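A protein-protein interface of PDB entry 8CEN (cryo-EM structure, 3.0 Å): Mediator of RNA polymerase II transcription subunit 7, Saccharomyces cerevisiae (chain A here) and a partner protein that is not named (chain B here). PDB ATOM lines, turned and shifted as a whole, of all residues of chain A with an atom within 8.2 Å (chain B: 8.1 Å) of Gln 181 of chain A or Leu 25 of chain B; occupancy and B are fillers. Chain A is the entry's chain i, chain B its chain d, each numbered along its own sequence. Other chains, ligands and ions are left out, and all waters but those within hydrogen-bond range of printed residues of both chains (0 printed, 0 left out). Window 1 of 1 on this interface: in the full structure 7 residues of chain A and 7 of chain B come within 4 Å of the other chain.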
ATOM      1  N   LEU A 174      -1.138  13.043  -5.547  1.00  0.00           N
ATOM      2  CA  LEU A 174      -1.157  14.502  -5.641  1.00  0.00           C
ATOM      3  C   LEU A 174      -2.246  15.101  -4.752  1.00  0.00           C
ATOM      4  O   LEU A 174      -2.028  16.130  -4.092  1.00  0.00           O
ATOM      5  CB  LEU A 174      -1.346  14.929  -7.096  1.00  0.00           C
ATOM      6  CG  LEU A 174      -1.533  16.422  -7.365  1.00  0.00           C
ATOM      7  CD1 LEU A 174      -0.257  17.180  -7.052  1.00  0.00           C
ATOM      8  CD2 LEU A 174      -1.949  16.651  -8.807  1.00  0.00           C
ATOM      9  N   ILE A 175      -3.422  14.465  -4.722  1.00  0.00           N
ATOM     10  CA  ILE A 175      -4.498  14.890  -3.828  1.00  0.00           C
ATOM     11  C   ILE A 175      -4.062  14.772  -2.371  1.00  0.00           C
ATOM     12  O   ILE A 175      -4.345  15.649  -1.549  1.00  0.00           O
ATOM     13  CB  ILE A 175      -5.774  14.076  -4.119  1.00  0.00           C
ATOM     14  CG1 ILE A 175      -6.410  14.533  -5.431  1.00  0.00           C
ATOM     15  CG2 ILE A 175      -6.790  14.196  -2.991  1.00  0.00           C
ATOM     16  CD1 ILE A 175      -7.554  13.662  -5.884  1.00  0.00           C
ATOM     17  N   MET A 176      -3.350  13.692  -2.038  1.00  0.00           N
ATOM     18  CA  MET A 176      -2.830  13.501  -0.687  1.00  0.00           C
ATOM     19  C   MET A 176      -1.792  14.559  -0.333  1.00  0.00           C
ATOM     20  O   MET A 176      -1.732  15.013   0.812  1.00  0.00           O
ATOM     21  CB  MET A 176      -2.235  12.099  -0.555  1.00  0.00           C
ATOM     22  CG  MET A 176      -1.769  11.739   0.846  1.00  0.00           C
ATOM     23  SD  MET A 176      -1.086  10.074   0.945  1.00  0.00           S
ATOM     24  CE  MET A 176      -2.571   9.087   0.782  1.00  0.00           C
ATOM     25  N   LEU A 177      -0.961  14.950  -1.303  1.00  0.00           N
ATOM     26  CA  LEU A 177      -0.001  16.030  -1.087  1.00  0.00           C
ATOM     27  C   LEU A 177      -0.707  17.345  -0.775  1.00  0.00           C
ATOM     28  O   LEU A 177      -0.331  18.058   0.166  1.00  0.00           O
ATOM     29  CB  LEU A 177       0.888  16.180  -2.321  1.00  0.00           C
ATOM     30  CG  LEU A 177       1.867  17.353  -2.326  1.00  0.00           C
ATOM     31  CD1 LEU A 177       2.911  17.190  -1.238  1.00  0.00           C
ATOM     32  CD2 LEU A 177       2.518  17.481  -3.689  1.00  0.00           C
ATOM     33  N   LEU A 178      -1.741  17.675  -1.555  1.00  0.00           N
ATOM     34  CA  LEU A 178      -2.519  18.885  -1.286  1.00  0.00           C
ATOM     35  C   LEU A 178      -3.219  18.816   0.068  1.00  0.00           C
ATOM     36  O   LEU A 178      -3.264  19.810   0.804  1.00  0.00           O
ATOM     37  CB  LEU A 178      -3.540  19.116  -2.397  1.00  0.00           C
ATOM     38  CG  LEU A 178      -3.054  19.648  -3.741  1.00  0.00           C
ATOM     39  CD1 LEU A 178      -4.158  19.540  -4.757  1.00  0.00           C
ATOM     40  CD2 LEU A 178      -2.659  21.094  -3.585  1.00  0.00           C
ATOM     41  N   GLU A 179      -3.766  17.649   0.414  1.00  0.00           N
ATOM     42  CA  GLU A 179      -4.459  17.493   1.689  1.00  0.00           C
ATOM     43  C   GLU A 179      -3.497  17.594   2.865  1.00  0.00           C
ATOM     44  O   GLU A 179      -3.846  18.150   3.909  1.00  0.00           O
ATOM     45  CB  GLU A 179      -5.206  16.160   1.718  1.00  0.00           C
ATOM     46  CG  GLU A 179      -6.589  16.210   1.094  1.00  0.00           C
ATOM     47  CD  GLU A 179      -7.181  14.831   0.882  1.00  0.00           C
ATOM     48  OE1 GLU A 179      -6.475  13.834   1.145  1.00  0.00           O
ATOM     49  OE2 GLU A 179      -8.350  14.743   0.451  1.00  0.00           O
ATOM     50  N   GLU A 180      -2.279  17.069   2.717  1.00  0.00           N
ATOM     51  CA  GLU A 180      -1.292  17.175   3.786  1.00  0.00           C
ATOM     52  C   GLU A 180      -0.773  18.599   3.931  1.00  0.00           C
ATOM     53  O   GLU A 180      -0.498  19.046   5.053  1.00  0.00           O
ATOM     54  CB  GLU A 180      -0.141  16.204   3.533  1.00  0.00           C
ATOM     55  CG  GLU A 180      -0.401  14.806   4.067  1.00  0.00           C
ATOM     56  CD  GLU A 180       0.855  13.965   4.138  1.00  0.00           C
ATOM     57  OE1 GLU A 180       1.597  14.085   5.136  1.00  0.00           O
ATOM     58  OE2 GLU A 180       1.095  13.181   3.198  1.00  0.00           O
ATOM     59  N   GLN A 181      -0.646  19.329   2.818  1.00  0.00           N
ATOM     60  CA  GLN A 181      -0.328  20.751   2.914  1.00  0.00           C
ATOM     61  C   GLN A 181      -1.441  21.518   3.617  1.00  0.00           C
ATOM     62  O   GLN A 181      -1.169  22.390   4.451  1.00  0.00           O
ATOM     63  CB  GLN A 181      -0.070  21.336   1.528  1.00  0.00           C
ATOM     64  CG  GLN A 181       1.250  20.916   0.919  1.00  0.00           C
ATOM     65  CD  GLN A 181       1.808  21.969  -0.009  1.00  0.00           C
ATOM     66  OE1 GLN A 181       1.169  22.990  -0.260  1.00  0.00           O
ATOM     67  NE2 GLN A 181       3.005  21.728  -0.528  1.00  0.00           N
ATOM     68  N   LEU A 182      -2.699  21.195   3.303  1.00  0.00           N
ATOM     69  CA  LEU A 182      -3.831  21.812   3.992  1.00  0.00           C
ATOM     70  C   LEU A 182      -3.832  21.470   5.476  1.00  0.00           C
ATOM     71  O   LEU A 182      -4.168  22.313   6.316  1.00  0.00           O
ATOM     72  CB  LEU A 182      -5.142  21.364   3.350  1.00  0.00           C
ATOM     73  CG  LEU A 182      -5.687  22.208   2.202  1.00  0.00           C
ATOM     74  CD1 LEU A 182      -6.916  21.556   1.619  1.00  0.00           C
ATOM     75  CD2 LEU A 182      -6.023  23.586   2.700  1.00  0.00           C
ATOM     76  N   GLU A 183      -3.475  20.228   5.813  1.00  0.00           N
ATOM     77  CA  GLU A 183      -3.417  19.810   7.208  1.00  0.00           C
ATOM     78  C   GLU A 183      -2.339  20.567   7.969  1.00  0.00           C
ATOM     79  O   GLU A 183      -2.566  21.003   9.103  1.00  0.00           O
ATOM     80  CB  GLU A 183      -3.177  18.302   7.291  1.00  0.00           C
ATOM     81  CG  GLU A 183      -3.313  17.727   8.690  1.00  0.00           C
ATOM     82  CD  GLU A 183      -4.672  17.999   9.303  1.00  0.00           C
ATOM     83  OE1 GLU A 183      -5.666  17.401   8.841  1.00  0.00           O
ATOM     84  OE2 GLU A 183      -4.746  18.809  10.252  1.00  0.00           O
ATOM     85  N   TYR A 184      -1.159  20.741   7.361  1.00  0.00           N
ATOM     86  CA  TYR A 184      -0.106  21.520   8.008  1.00  0.00           C
ATOM     87  C   TYR A 184      -0.516  22.981   8.149  1.00  0.00           C
ATOM     88  O   TYR A 184      -0.229  23.614   9.174  1.00  0.00           O
ATOM     89  CB  TYR A 184       1.208  21.395   7.231  1.00  0.00           C
ATOM     90  CG  TYR A 184       2.377  22.165   7.828  1.00  0.00           C
ATOM     91  CD1 TYR A 184       2.627  23.493   7.484  1.00  0.00           C
ATOM     92  CD2 TYR A 184       3.232  21.556   8.737  1.00  0.00           C
ATOM     93  CE1 TYR A 184       3.687  24.188   8.037  1.00  0.00           C
ATOM     94  CE2 TYR A 184       4.298  22.243   9.289  1.00  0.00           C
ATOM     95  CZ  TYR A 184       4.521  23.557   8.935  1.00  0.00           C
ATOM     96  OH  TYR A 184       5.581  24.244   9.482  1.00  0.00           O
ATOM     97  N   LYS A 185      -1.175  23.533   7.124  1.00  0.00           N
ATOM     98  CA  LYS A 185      -1.646  24.913   7.186  1.00  0.00           C
ATOM     99  C   LYS A 185      -2.640  25.106   8.325  1.00  0.00           C
ATOM    100  O   LYS A 185      -2.508  26.038   9.126  1.00  0.00           O
ATOM    101  CB  LYS A 185      -2.283  25.308   5.853  1.00  0.00           C
ATOM    102  CG  LYS A 185      -1.298  25.613   4.736  1.00  0.00           C
ATOM    103  CD  LYS A 185      -0.445  26.820   5.053  1.00  0.00           C
ATOM    104  CE  LYS A 185       0.817  26.837   4.209  1.00  0.00           C
ATOM    105  NZ  LYS A 185       1.710  25.691   4.521  1.00  0.00           N
ATOM    106  N   ARG A 186      -3.623  24.208   8.434  1.00  0.00           N
ATOM    107  CA  ARG A 186      -4.612  24.314   9.501  1.00  0.00           C
ATOM    108  C   ARG A 186      -4.009  24.036  10.872  1.00  0.00           C
ATOM    109  O   ARG A 186      -4.464  24.609  11.867  1.00  0.00           O
ATOM    110  CB  ARG A 186      -5.786  23.373   9.238  1.00  0.00           C
ATOM    111  CG  ARG A 186      -6.729  23.855   8.153  1.00  0.00           C
ATOM    112  CD  ARG A 186      -7.906  22.910   7.997  1.00  0.00           C
ATOM    113  NE  ARG A 186      -8.899  23.443   7.074  1.00  0.00           N
ATOM    114  CZ  ARG A 186      -8.921  23.204   5.770  1.00  0.00           C
ATOM    115  NH1 ARG A 186      -8.036  22.404   5.200  1.00  0.00           N
ATOM    116  NH2 ARG A 186      -9.856  23.780   5.023  1.00  0.00           N
ATOM    117  N   GLY A 187      -2.994  23.173  10.949  1.00  0.00           N
ATOM    118  CA  GLY A 187      -2.286  22.996  12.206  1.00  0.00           C
ATOM    119  C   GLY A 187      -1.550  24.250  12.633  1.00  0.00           C
ATOM    120  O   GLY A 187      -1.514  24.589  13.821  1.00  0.00           O
ATOM    121  N   GLU A 188      -0.960  24.963  11.668  1.00  0.00           N
ATOM    122  CA  GLU A 188      -0.344  26.250  11.972  1.00  0.00           C
ATOM    123  C   GLU A 188      -1.385  27.272  12.413  1.00  0.00           C
ATOM    124  O   GLU A 188      -1.130  28.063  13.328  1.00  0.00           O
ATOM    125  CB  GLU A 188       0.450  26.756  10.769  1.00  0.00           C
ATOM    126  CG  GLU A 188       1.895  26.277  10.760  1.00  0.00           C
ATOM    127  CD  GLU A 188       2.799  27.139   9.902  1.00  0.00           C
ATOM    128  OE1 GLU A 188       2.361  27.562   8.813  1.00  0.00           O
ATOM    129  OE2 GLU A 188       3.947  27.399  10.319  1.00  0.00           O
ATOM    130  N   ALA B  20      -1.852  25.728  -7.333  1.00  0.00           N
ATOM    131  CA  ALA B  20      -1.232  26.589  -6.335  1.00  0.00           C
ATOM    132  C   ALA B  20      -0.708  25.708  -5.211  1.00  0.00           C
ATOM    133  O   ALA B  20      -1.474  24.953  -4.601  1.00  0.00           O
ATOM    134  CB  ALA B  20      -2.226  27.617  -5.797  1.00  0.00           C
ATOM    135  N   LEU B  21       0.591  25.798  -4.943  1.00  0.00           N
ATOM    136  CA  LEU B  21       1.246  24.911  -3.997  1.00  0.00           C
ATOM    137  C   LEU B  21       2.255  25.688  -3.169  1.00  0.00           C
ATOM    138  O   LEU B  21       2.763  26.728  -3.595  1.00  0.00           O
ATOM    139  CB  LEU B  21       1.940  23.750  -4.720  1.00  0.00           C
ATOM    140  CG  LEU B  21       1.133  22.456  -4.787  1.00  0.00           C
ATOM    141  CD1 LEU B  21       1.885  21.386  -5.532  1.00  0.00           C
ATOM    142  CD2 LEU B  21       0.856  21.993  -3.383  1.00  0.00           C
ATOM    143  N   ASP B  22       2.528  25.176  -1.973  1.00  0.00           N
ATOM    144  CA  ASP B  22       3.604  25.697  -1.143  1.00  0.00           C
ATOM    145  C   ASP B  22       4.851  24.859  -1.397  1.00  0.00           C
ATOM    146  O   ASP B  22       4.958  23.738  -0.886  1.00  0.00           O
ATOM    147  CB  ASP B  22       3.218  25.669   0.336  1.00  0.00           C
ATOM    148  CG  ASP B  22       3.975  26.694   1.158  1.00  0.00           C
ATOM    149  OD1 ASP B  22       5.044  27.158   0.707  1.00  0.00           O
ATOM    150  OD2 ASP B  22       3.501  27.037   2.261  1.00  0.00           O
ATOM    151  N   PRO B  23       5.812  25.365  -2.175  1.00  0.00           N
ATOM    152  CA  PRO B  23       6.976  24.542  -2.533  1.00  0.00           C
ATOM    153  C   PRO B  23       7.977  24.367  -1.406  1.00  0.00           C
ATOM    154  O   PRO B  23       8.882  23.535  -1.542  1.00  0.00           O
ATOM    155  CB  PRO B  23       7.594  25.304  -3.708  1.00  0.00           C
ATOM    156  CG  PRO B  23       7.209  26.718  -3.480  1.00  0.00           C
ATOM    157  CD  PRO B  23       5.921  26.738  -2.697  1.00  0.00           C
ATOM    158  N   ASN B  24       7.843  25.116  -0.308  1.00  0.00           N
ATOM    159  CA  ASN B  24       8.789  25.000   0.797  1.00  0.00           C
ATOM    160  C   ASN B  24       8.720  23.632   1.464  1.00  0.00           C
ATOM    161  O   ASN B  24       9.733  23.139   1.971  1.00  0.00           O
ATOM    162  CB  ASN B  24       8.532  26.102   1.825  1.00  0.00           C
ATOM    163  CG  ASN B  24       8.705  27.489   1.244  1.00  0.00           C
ATOM    164  OD1 ASN B  24       9.609  27.728   0.445  1.00  0.00           O
ATOM    165  ND2 ASN B  24       7.835  28.410   1.639  1.00  0.00           N
ATOM    166  N   LEU B  25       7.545  23.007   1.474  1.00  0.00           N
ATOM    167  CA  LEU B  25       7.365  21.691   2.076  1.00  0.00           C
ATOM    168  C   LEU B  25       6.660  20.788   1.072  1.00  0.00           C
ATOM    169  O   LEU B  25       5.576  21.118   0.581  1.00  0.00           O
ATOM    170  CB  LEU B  25       6.614  21.805   3.408  1.00  0.00           C
ATOM    171  CG  LEU B  25       5.193  22.354   3.607  1.00  0.00           C
ATOM    172  CD1 LEU B  25       4.069  21.347   3.361  1.00  0.00           C
ATOM    173  CD2 LEU B  25       5.091  22.955   4.987  1.00  0.00           C
ATOM    174  N   ILE B  26       7.319  19.689   0.702  1.00  0.00           N
ATOM    175  CA  ILE B  26       6.763  18.727  -0.241  1.00  0.00           C
ATOM    176  C   ILE B  26       6.714  17.361   0.433  1.00  0.00           C
ATOM    177  O   ILE B  26       5.852  16.530   0.127  1.00  0.00           O
ATOM    178  CB  ILE B  26       7.589  18.674  -1.542  1.00  0.00           C
ATOM    179  CG1 ILE B  26       7.893  20.086  -2.052  1.00  0.00           C
ATOM    180  CG2 ILE B  26       6.850  17.904  -2.622  1.00  0.00           C
ATOM    181  CD1 ILE B  26       6.678  20.839  -2.531  1.00  0.00           C
ATOM    182  N   THR B  27       7.626  17.130   1.372  1.00  0.00           N
ATOM    183  CA  THR B  27       7.723  15.830   2.019  1.00  0.00           C
ATOM    184  C   THR B  27       6.609  15.646   3.046  1.00  0.00           C
ATOM    185  O   THR B  27       6.199  16.586   3.732  1.00  0.00           O
ATOM    186  CB  THR B  27       9.084  15.667   2.694  1.00  0.00           C
ATOM    187  OG1 THR B  27       9.240  16.672   3.704  1.00  0.00           O
ATOM    188  CG2 THR B  27      10.204  15.807   1.673  1.00  0.00           C
ATOM    189  N   LEU B  28       6.122  14.412   3.145  1.00  0.00           N
ATOM    190  CA  LEU B  28       5.092  14.068   4.110  1.00  0.00           C
ATOM    191  C   LEU B  28       5.707  13.848   5.491  1.00  0.00           C
ATOM    192  O   LEU B  28       6.925  13.729   5.650  1.00  0.00           O
ATOM    193  CB  LEU B  28       4.320  12.820   3.670  1.00  0.00           C
ATOM    194  CG  LEU B  28       4.939  11.418   3.757  1.00  0.00           C
ATOM    195  CD1 LEU B  28       3.842  10.370   3.653  1.00  0.00           C
ATOM    196  CD2 LEU B  28       5.991  11.165   2.684  1.00  0.00           C
ATOM    197  N   SER B  85      12.024  25.171   1.820  1.00  0.00           N
ATOM    198  CA  SER B  85      13.412  24.731   1.798  1.00  0.00           C
ATOM    199  C   SER B  85      14.045  24.987   0.435  1.00  0.00           C
ATOM    200  O   SER B  85      15.108  25.601   0.341  1.00  0.00           O
ATOM    201  CB  SER B  85      13.511  23.246   2.154  1.00  0.00           C
ATOM    202  OG  SER B  85      14.860  22.814   2.163  1.00  0.00           O
ATOM    203  N   LEU B  86      13.387  24.506  -0.624  1.00  0.00           N
ATOM    204  CA  LEU B  86      13.908  24.719  -1.970  1.00  0.00           C
ATOM    205  C   LEU B  86      13.733  26.166  -2.418  1.00  0.00           C
ATOM    206  O   LEU B  86      14.574  26.689  -3.157  1.00  0.00           O
ATOM    207  CB  LEU B  86      13.253  23.733  -2.944  1.00  0.00           C
ATOM    208  CG  LEU B  86      11.734  23.677  -3.144  1.00  0.00           C
ATOM    209  CD1 LEU B  86      11.223  24.632  -4.215  1.00  0.00           C
ATOM    210  CD2 LEU B  86      11.293  22.253  -3.443  1.00  0.00           C
ATOM    211  N   VAL B  87      12.663  26.827  -1.988  1.00  0.00           N
ATOM    212  CA  VAL B  87      12.528  28.270  -2.148  1.00  0.00           C
ATOM    213  C   VAL B  87      13.085  28.927  -0.894  1.00  0.00           C
ATOM    214  O   VAL B  87      12.615  28.662   0.219  1.00  0.00           O
ATOM    215  CB  VAL B  87      11.068  28.680  -2.392  1.00  0.00           C
ATOM    216  CG1 VAL B  87      10.907  30.183  -2.225  1.00  0.00           C
ATOM    217  CG2 VAL B  87      10.627  28.262  -3.782  1.00  0.00           C
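Among the printed residues, merely in contact across the chains: Glu 180 of chain A with Leu 28 of chain B (3.3 Å), Gln 181 of chain A with Leu 21 of chain B (3.3 Å), Leu 177 of chain A with Ile 26 of chain B (3.3 Å), Tyr 184 of chain A with Leu 25 of chain B (3.5 Å) and Leu 178 of chain A with Leu 21 of chain B (3.6 Å).
ND2 of Asn 24 of chain B is in hydrogen-bond range of OD1 of Asp 22 of chain B (3.2 Å).
Of the 12 printed residues of chain B, 5 touch a printed residue of chain A.
Printed residues of chain B that touch a printed residue of chain A: Leu 21, Asp 22, Leu 25, Ile 26 and Leu 28.
Hydrophobic or aromatic side chains of chain B within 4 Å of the printed part of chain A: Leu 21, Leu 25 and Leu 28.
Among the printed residues, 8 pairs touch across the chains.
Glu 179 of chain A touches none of the printed residues of chain B.
Of the printed residues of chain B, Glu 180 of chain A touches Leu 28 (3.3 Å).
Gln 181 of chain A touches just these residues of chain B: Leu 21, Asp 22 and Leu 25.
Printed residues of chain B within 4 Å of Tyr 184 of chain A: Leu 25 (3.5 Å).
Of the printed residues of chain A, Leu 21 of chain B touches Leu 178 and Gln 181.
Printed residues of chain A within 4 Å of Asp 22 of chain B: Gln 181 and Lys 185.
Pro 23 of chain B touches none of the printed residues of chain A.
Leu 25 of chain B touches just these residues of chain A: Gln 181 and Tyr 184.
Printed residues of chain A within 4 Å of Leu 28 of chain B: Glu 180 (3.3 Å).
The nearest residue of chain B that does not touch Gln 181 of chain A is Ile 26 of chain B (4.3 Å).
The nearest printed residue of chain B that does not touch Lys 185 of chain A is Leu 25 of chain B (4.4 Å).
O of Asp 22 of chain B is in hydrogen-bond range of NE2 of Gln 181 of chain A.
OD2 of Asp 22 of chain B lies within salt-bridge range of NZ of Lys 185 of chain A, at 3.2 Å.
NE2 of Gln 181 of chain A sits at hydrogen-bond distance from O of Leu 25 of chain B (2.9 Å).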
